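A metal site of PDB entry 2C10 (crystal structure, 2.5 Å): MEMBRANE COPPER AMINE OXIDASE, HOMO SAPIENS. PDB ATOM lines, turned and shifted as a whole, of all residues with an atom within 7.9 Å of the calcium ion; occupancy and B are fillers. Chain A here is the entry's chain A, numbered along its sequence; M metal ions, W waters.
Water W1 bridges the side-chain carboxylate of Glu 613 (2.5 Å) and the side-chain amino group of Lys 610 (3.2 Å).
The backbone NH of Gln 608 sits close to the side-chain carboxylate of Glu 544 (3.0 Å).
The side-chain carboxylate (OE2) of Glu 639 lies within salt-bridge range of the side-chain amino group (NZ) of Lys 610 (2.8 Å).
The calcium ion is bound by O of Phe 635 (2.3 Å).
OD1 of Asn 637 binds the calcium ion (2.4 Å).
OE2 of Glu 544 binds the calcium ion (2.5 Å).
The calcium ion is bound by water W1 (2.5 Å).
OE1 of Glu 544 is bound to the calcium ion, 2.6 Å away.
The calcium ion is bound by OE1 of Glu 639 (2.6 Å).
The calcium ion has six donor atoms within binding distance.
Within 4 Å of the calcium ion: Glu 544, Phe 635, Asn 637 and Glu 639.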
ATOM      1  N   GLU A 544     -29.354 -14.370   8.672  1.00  0.00           N
ATOM      2  CA  GLU A 544     -29.220 -14.687  10.098  1.00  0.00           C
ATOM      3  C   GLU A 544     -30.120 -13.842  11.002  1.00  0.00           C
ATOM      4  O   GLU A 544     -30.716 -14.366  11.939  1.00  0.00           O
ATOM      5  CB  GLU A 544     -27.756 -14.557  10.543  1.00  0.00           C
ATOM      6  CG  GLU A 544     -26.887 -15.732  10.081  1.00  0.00           C
ATOM      7  CD  GLU A 544     -25.392 -15.581  10.375  1.00  0.00           C
ATOM      8  OE1 GLU A 544     -24.652 -16.574  10.171  1.00  0.00           O
ATOM      9  OE2 GLU A 544     -24.939 -14.498  10.812  1.00  0.00           O
ATOM     10  N   VAL A 606     -30.154 -18.834  14.436  1.00  0.00           N
ATOM     11  CA  VAL A 606     -29.628 -19.751  13.453  1.00  0.00           C
ATOM     12  C   VAL A 606     -28.543 -19.031  12.682  1.00  0.00           C
ATOM     13  O   VAL A 606     -28.763 -17.954  12.127  1.00  0.00           O
ATOM     14  CB  VAL A 606     -30.731 -20.313  12.487  1.00  0.00           C
ATOM     15  CG1 VAL A 606     -30.159 -21.415  11.628  1.00  0.00           C
ATOM     16  CG2 VAL A 606     -31.915 -20.868  13.265  1.00  0.00           C
ATOM     17  N   THR A 607     -27.350 -19.624  12.663  1.00  0.00           N
ATOM     18  CA  THR A 607     -26.186 -19.022  12.023  1.00  0.00           C
ATOM     19  C   THR A 607     -25.509 -20.049  11.105  1.00  0.00           C
ATOM     20  O   THR A 607     -25.774 -21.261  11.204  1.00  0.00           O
ATOM     21  CB  THR A 607     -25.151 -18.566  13.082  1.00  0.00           C
ATOM     22  OG1 THR A 607     -24.674 -19.696  13.820  1.00  0.00           O
ATOM     23  CG2 THR A 607     -25.755 -17.559  14.069  1.00  0.00           C
ATOM     24  N   GLN A 608     -24.647 -19.586  10.211  1.00  0.00           N
ATOM     25  CA  GLN A 608     -23.756 -20.486   9.499  1.00  0.00           C
ATOM     26  C   GLN A 608     -22.828 -21.144  10.516  1.00  0.00           C
ATOM     27  O   GLN A 608     -22.211 -20.462  11.334  1.00  0.00           O
ATOM     28  CB  GLN A 608     -22.928 -19.719   8.464  1.00  0.00           C
ATOM     29  CG  GLN A 608     -23.744 -19.082   7.346  1.00  0.00           C
ATOM     30  CD  GLN A 608     -22.902 -18.454   6.252  1.00  0.00           C
ATOM     31  OE1 GLN A 608     -21.676 -18.639   6.191  1.00  0.00           O
ATOM     32  NE2 GLN A 608     -23.549 -17.700   5.362  1.00  0.00           N
ATOM     33  N   ARG A 609     -22.755 -22.475  10.474  1.00  0.00           N
ATOM     34  CA  ARG A 609     -21.760 -23.197  11.256  1.00  0.00           C
ATOM     35  C   ARG A 609     -20.379 -22.931  10.660  1.00  0.00           C
ATOM     36  O   ARG A 609     -20.155 -23.122   9.455  1.00  0.00           O
ATOM     37  CB  ARG A 609     -22.165 -24.688  11.436  1.00  0.00           C
ATOM     38  CG  ARG A 609     -21.161 -25.852  11.168  1.00  0.00           C
ATOM     39  CD  ARG A 609     -19.915 -25.776  11.967  1.00  0.00           C
ATOM     40  NE  ARG A 609     -19.589 -26.996  12.706  1.00  0.00           N
ATOM     41  CZ  ARG A 609     -18.376 -27.553  12.716  1.00  0.00           C
ATOM     42  NH1 ARG A 609     -18.152 -28.638  13.459  1.00  0.00           N
ATOM     43  NH2 ARG A 609     -17.396 -27.032  12.003  1.00  0.00           N
ATOM     44  N   LYS A 610     -19.487 -22.403  11.494  1.00  0.00           N
ATOM     45  CA  LYS A 610     -18.111 -22.075  11.085  1.00  0.00           C
ATOM     46  C   LYS A 610     -17.125 -22.721  12.053  1.00  0.00           C
ATOM     47  O   LYS A 610     -17.408 -22.839  13.253  1.00  0.00           O
ATOM     48  CB  LYS A 610     -17.875 -20.550  11.083  1.00  0.00           C
ATOM     49  CG  LYS A 610     -18.854 -19.732  10.244  1.00  0.00           C
ATOM     50  CD  LYS A 610     -18.436 -18.264  10.222  1.00  0.00           C
ATOM     51  CE  LYS A 610     -19.097 -17.539   9.056  1.00  0.00           C
ATOM     52  NZ  LYS A 610     -19.049 -16.062   9.182  1.00  0.00           N
ATOM     53  N   GLU A 613     -16.138 -20.700  15.052  1.00  0.00           N
ATOM     54  CA  GLU A 613     -17.244 -20.369  15.961  1.00  0.00           C
ATOM     55  C   GLU A 613     -17.789 -21.639  16.589  1.00  0.00           C
ATOM     56  O   GLU A 613     -18.954 -21.992  16.361  1.00  0.00           O
ATOM     57  CB  GLU A 613     -18.357 -19.608  15.223  1.00  0.00           C
ATOM     58  CG  GLU A 613     -17.994 -18.180  14.814  1.00  0.00           C
ATOM     59  CD  GLU A 613     -19.111 -17.474  14.046  1.00  0.00           C
ATOM     60  OE1 GLU A 613     -20.165 -18.095  13.762  1.00  0.00           O
ATOM     61  OE2 GLU A 613     -18.941 -16.280  13.726  1.00  0.00           O
ATOM     62  N   PHE A 632     -21.192 -14.042  21.789  1.00  0.00           N
ATOM     63  CA  PHE A 632     -22.105 -14.790  20.919  1.00  0.00           C
ATOM     64  C   PHE A 632     -22.771 -13.927  19.858  1.00  0.00           C
ATOM     65  O   PHE A 632     -22.889 -14.349  18.708  1.00  0.00           O
ATOM     66  CB  PHE A 632     -23.162 -15.551  21.726  1.00  0.00           C
ATOM     67  CG  PHE A 632     -24.223 -16.226  20.871  1.00  0.00           C
ATOM     68  CD1 PHE A 632     -23.952 -17.429  20.221  1.00  0.00           C
ATOM     69  CD2 PHE A 632     -25.479 -15.654  20.718  1.00  0.00           C
ATOM     70  CE1 PHE A 632     -24.927 -18.055  19.440  1.00  0.00           C
ATOM     71  CE2 PHE A 632     -26.451 -16.266  19.923  1.00  0.00           C
ATOM     72  CZ  PHE A 632     -26.164 -17.471  19.289  1.00  0.00           C
ATOM     73  N   SER A 633     -23.201 -12.718  20.238  1.00  0.00           N
ATOM     74  CA  SER A 633     -23.900 -11.826  19.305  1.00  0.00           C
ATOM     75  C   SER A 633     -23.079 -11.514  18.056  1.00  0.00           C
ATOM     76  O   SER A 633     -23.626 -11.124  17.032  1.00  0.00           O
ATOM     77  CB  SER A 633     -24.375 -10.543  19.980  1.00  0.00           C
ATOM     78  OG  SER A 633     -23.280  -9.849  20.533  1.00  0.00           O
ATOM     79  N   ASP A 634     -21.758 -11.692  18.160  1.00  0.00           N
ATOM     80  CA  ASP A 634     -20.887 -11.538  16.991  1.00  0.00           C
ATOM     81  C   ASP A 634     -21.174 -12.563  15.892  1.00  0.00           C
ATOM     82  O   ASP A 634     -20.972 -12.274  14.725  1.00  0.00           O
ATOM     83  CB  ASP A 634     -19.407 -11.597  17.383  1.00  0.00           C
ATOM     84  CG  ASP A 634     -18.975 -10.371  18.181  1.00  0.00           C
ATOM     85  OD1 ASP A 634     -17.759 -10.282  18.521  1.00  0.00           O
ATOM     86  OD2 ASP A 634     -19.842  -9.507  18.468  1.00  0.00           O
ATOM     87  N   PHE A 635     -21.643 -13.758  16.260  1.00  0.00           N
ATOM     88  CA  PHE A 635     -21.947 -14.789  15.256  1.00  0.00           C
ATOM     89  C   PHE A 635     -23.091 -14.377  14.354  1.00  0.00           C
ATOM     90  O   PHE A 635     -23.260 -14.917  13.274  1.00  0.00           O
ATOM     91  CB  PHE A 635     -22.321 -16.139  15.897  1.00  0.00           C
ATOM     92  CG  PHE A 635     -21.277 -16.700  16.822  1.00  0.00           C
ATOM     93  CD1 PHE A 635     -20.063 -16.065  17.025  1.00  0.00           C
ATOM     94  CD2 PHE A 635     -21.513 -17.903  17.477  1.00  0.00           C
ATOM     95  CE1 PHE A 635     -19.105 -16.602  17.881  1.00  0.00           C
ATOM     96  CE2 PHE A 635     -20.564 -18.443  18.328  1.00  0.00           C
ATOM     97  CZ  PHE A 635     -19.357 -17.780  18.529  1.00  0.00           C
ATOM     98  N   ILE A 636     -23.905 -13.429  14.821  1.00  0.00           N
ATOM     99  CA  ILE A 636     -25.038 -12.932  14.045  1.00  0.00           C
ATOM    100  C   ILE A 636     -24.648 -11.658  13.310  1.00  0.00           C
ATOM    101  O   ILE A 636     -24.476 -10.599  13.923  1.00  0.00           O
ATOM    102  CB  ILE A 636     -26.298 -12.718  14.910  1.00  0.00           C
ATOM    103  CG1 ILE A 636     -26.577 -13.947  15.781  1.00  0.00           C
ATOM    104  CG2 ILE A 636     -27.497 -12.398  14.029  1.00  0.00           C
ATOM    105  CD1 ILE A 636     -27.529 -13.707  16.928  1.00  0.00           C
ATOM    106  N   ASN A 637     -24.487 -11.785  11.994  1.00  0.00           N
ATOM    107  CA  ASN A 637     -24.284 -10.657  11.100  1.00  0.00           C
ATOM    108  C   ASN A 637     -25.207 -10.757   9.885  1.00  0.00           C
ATOM    109  O   ASN A 637     -26.220 -11.449   9.924  1.00  0.00           O
ATOM    110  CB  ASN A 637     -22.809 -10.501  10.691  1.00  0.00           C
ATOM    111  CG  ASN A 637     -22.070 -11.832  10.582  1.00  0.00           C
ATOM    112  OD1 ASN A 637     -22.631 -12.920  10.699  1.00  0.00           O
ATOM    113  ND2 ASN A 637     -20.776 -11.731  10.354  1.00  0.00           N
ATOM    114  N   ASN A 638     -24.870 -10.070   8.797  1.00  0.00           N
ATOM    115  CA  ASN A 638     -25.761 -10.041   7.626  1.00  0.00           C
ATOM    116  C   ASN A 638     -25.622 -11.239   6.679  1.00  0.00           C
ATOM    117  O   ASN A 638     -25.827 -11.102   5.475  1.00  0.00           O
ATOM    118  CB  ASN A 638     -25.576  -8.727   6.855  1.00  0.00           C
ATOM    119  CG  ASN A 638     -26.477  -7.602   7.361  1.00  0.00           C
ATOM    120  OD1 ASN A 638     -26.682  -6.589   6.664  1.00  0.00           O
ATOM    121  ND2 ASN A 638     -27.015  -7.763   8.573  1.00  0.00           N
ATOM    122  N   GLU A 639     -25.263 -12.415   7.189  1.00  0.00           N
ATOM    123  CA  GLU A 639     -24.922 -13.514   6.295  1.00  0.00           C
ATOM    124  C   GLU A 639     -26.157 -14.294   5.869  1.00  0.00           C
ATOM    125  O   GLU A 639     -27.193 -14.252   6.553  1.00  0.00           O
ATOM    126  CB  GLU A 639     -23.910 -14.453   6.950  1.00  0.00           C
ATOM    127  CG  GLU A 639     -22.638 -13.768   7.445  1.00  0.00           C
ATOM    128  CD  GLU A 639     -21.543 -14.756   7.810  1.00  0.00           C
ATOM    129  OE1 GLU A 639     -21.800 -15.724   8.567  1.00  0.00           O
ATOM    130  OE2 GLU A 639     -20.413 -14.547   7.333  1.00  0.00           O
ATOM    131  N   THR A 640     -26.058 -14.994   4.753  1.00  0.00           N
ATOM    132  CA  THR A 640     -27.139 -15.868   4.291  1.00  0.00           C
ATOM    133  C   THR A 640     -27.280 -17.151   5.135  1.00  0.00           C
ATOM    134  O   THR A 640     -26.307 -17.676   5.663  1.00  0.00           O
ATOM    135  CB  THR A 640     -27.038 -16.199   2.767  1.00  0.00           C
ATOM    136  OG1 THR A 640     -28.172 -16.966   2.365  1.00  0.00           O
ATOM    137  CG2 THR A 640     -25.758 -16.945   2.421  1.00  0.00           C
ATOM    138  N   ILE A 641     -28.515 -17.609   5.257  1.00  0.00           N
ATOM    139  CA  ILE A 641     -28.823 -18.893   5.850  1.00  0.00           C
ATOM    140  C   ILE A 641     -29.704 -19.677   4.858  1.00  0.00           C
ATOM    141  O   ILE A 641     -30.522 -20.522   5.241  1.00  0.00           O
ATOM    142  CB  ILE A 641     -29.490 -18.759   7.263  1.00  0.00           C
ATOM    143  CG1 ILE A 641     -30.719 -17.859   7.205  1.00  0.00           C
ATOM    144  CG2 ILE A 641     -28.476 -18.238   8.283  1.00  0.00           C
ATOM    145  CD1 ILE A 641     -31.633 -17.987   8.394  1.00  0.00           C
HETATM  146 CA    CA M   1     -22.569 -15.303  11.066  1.00  0.00          CA
HETATM  147  O   HOH W   1     -20.220 -15.088  11.979  1.00  0.00           O
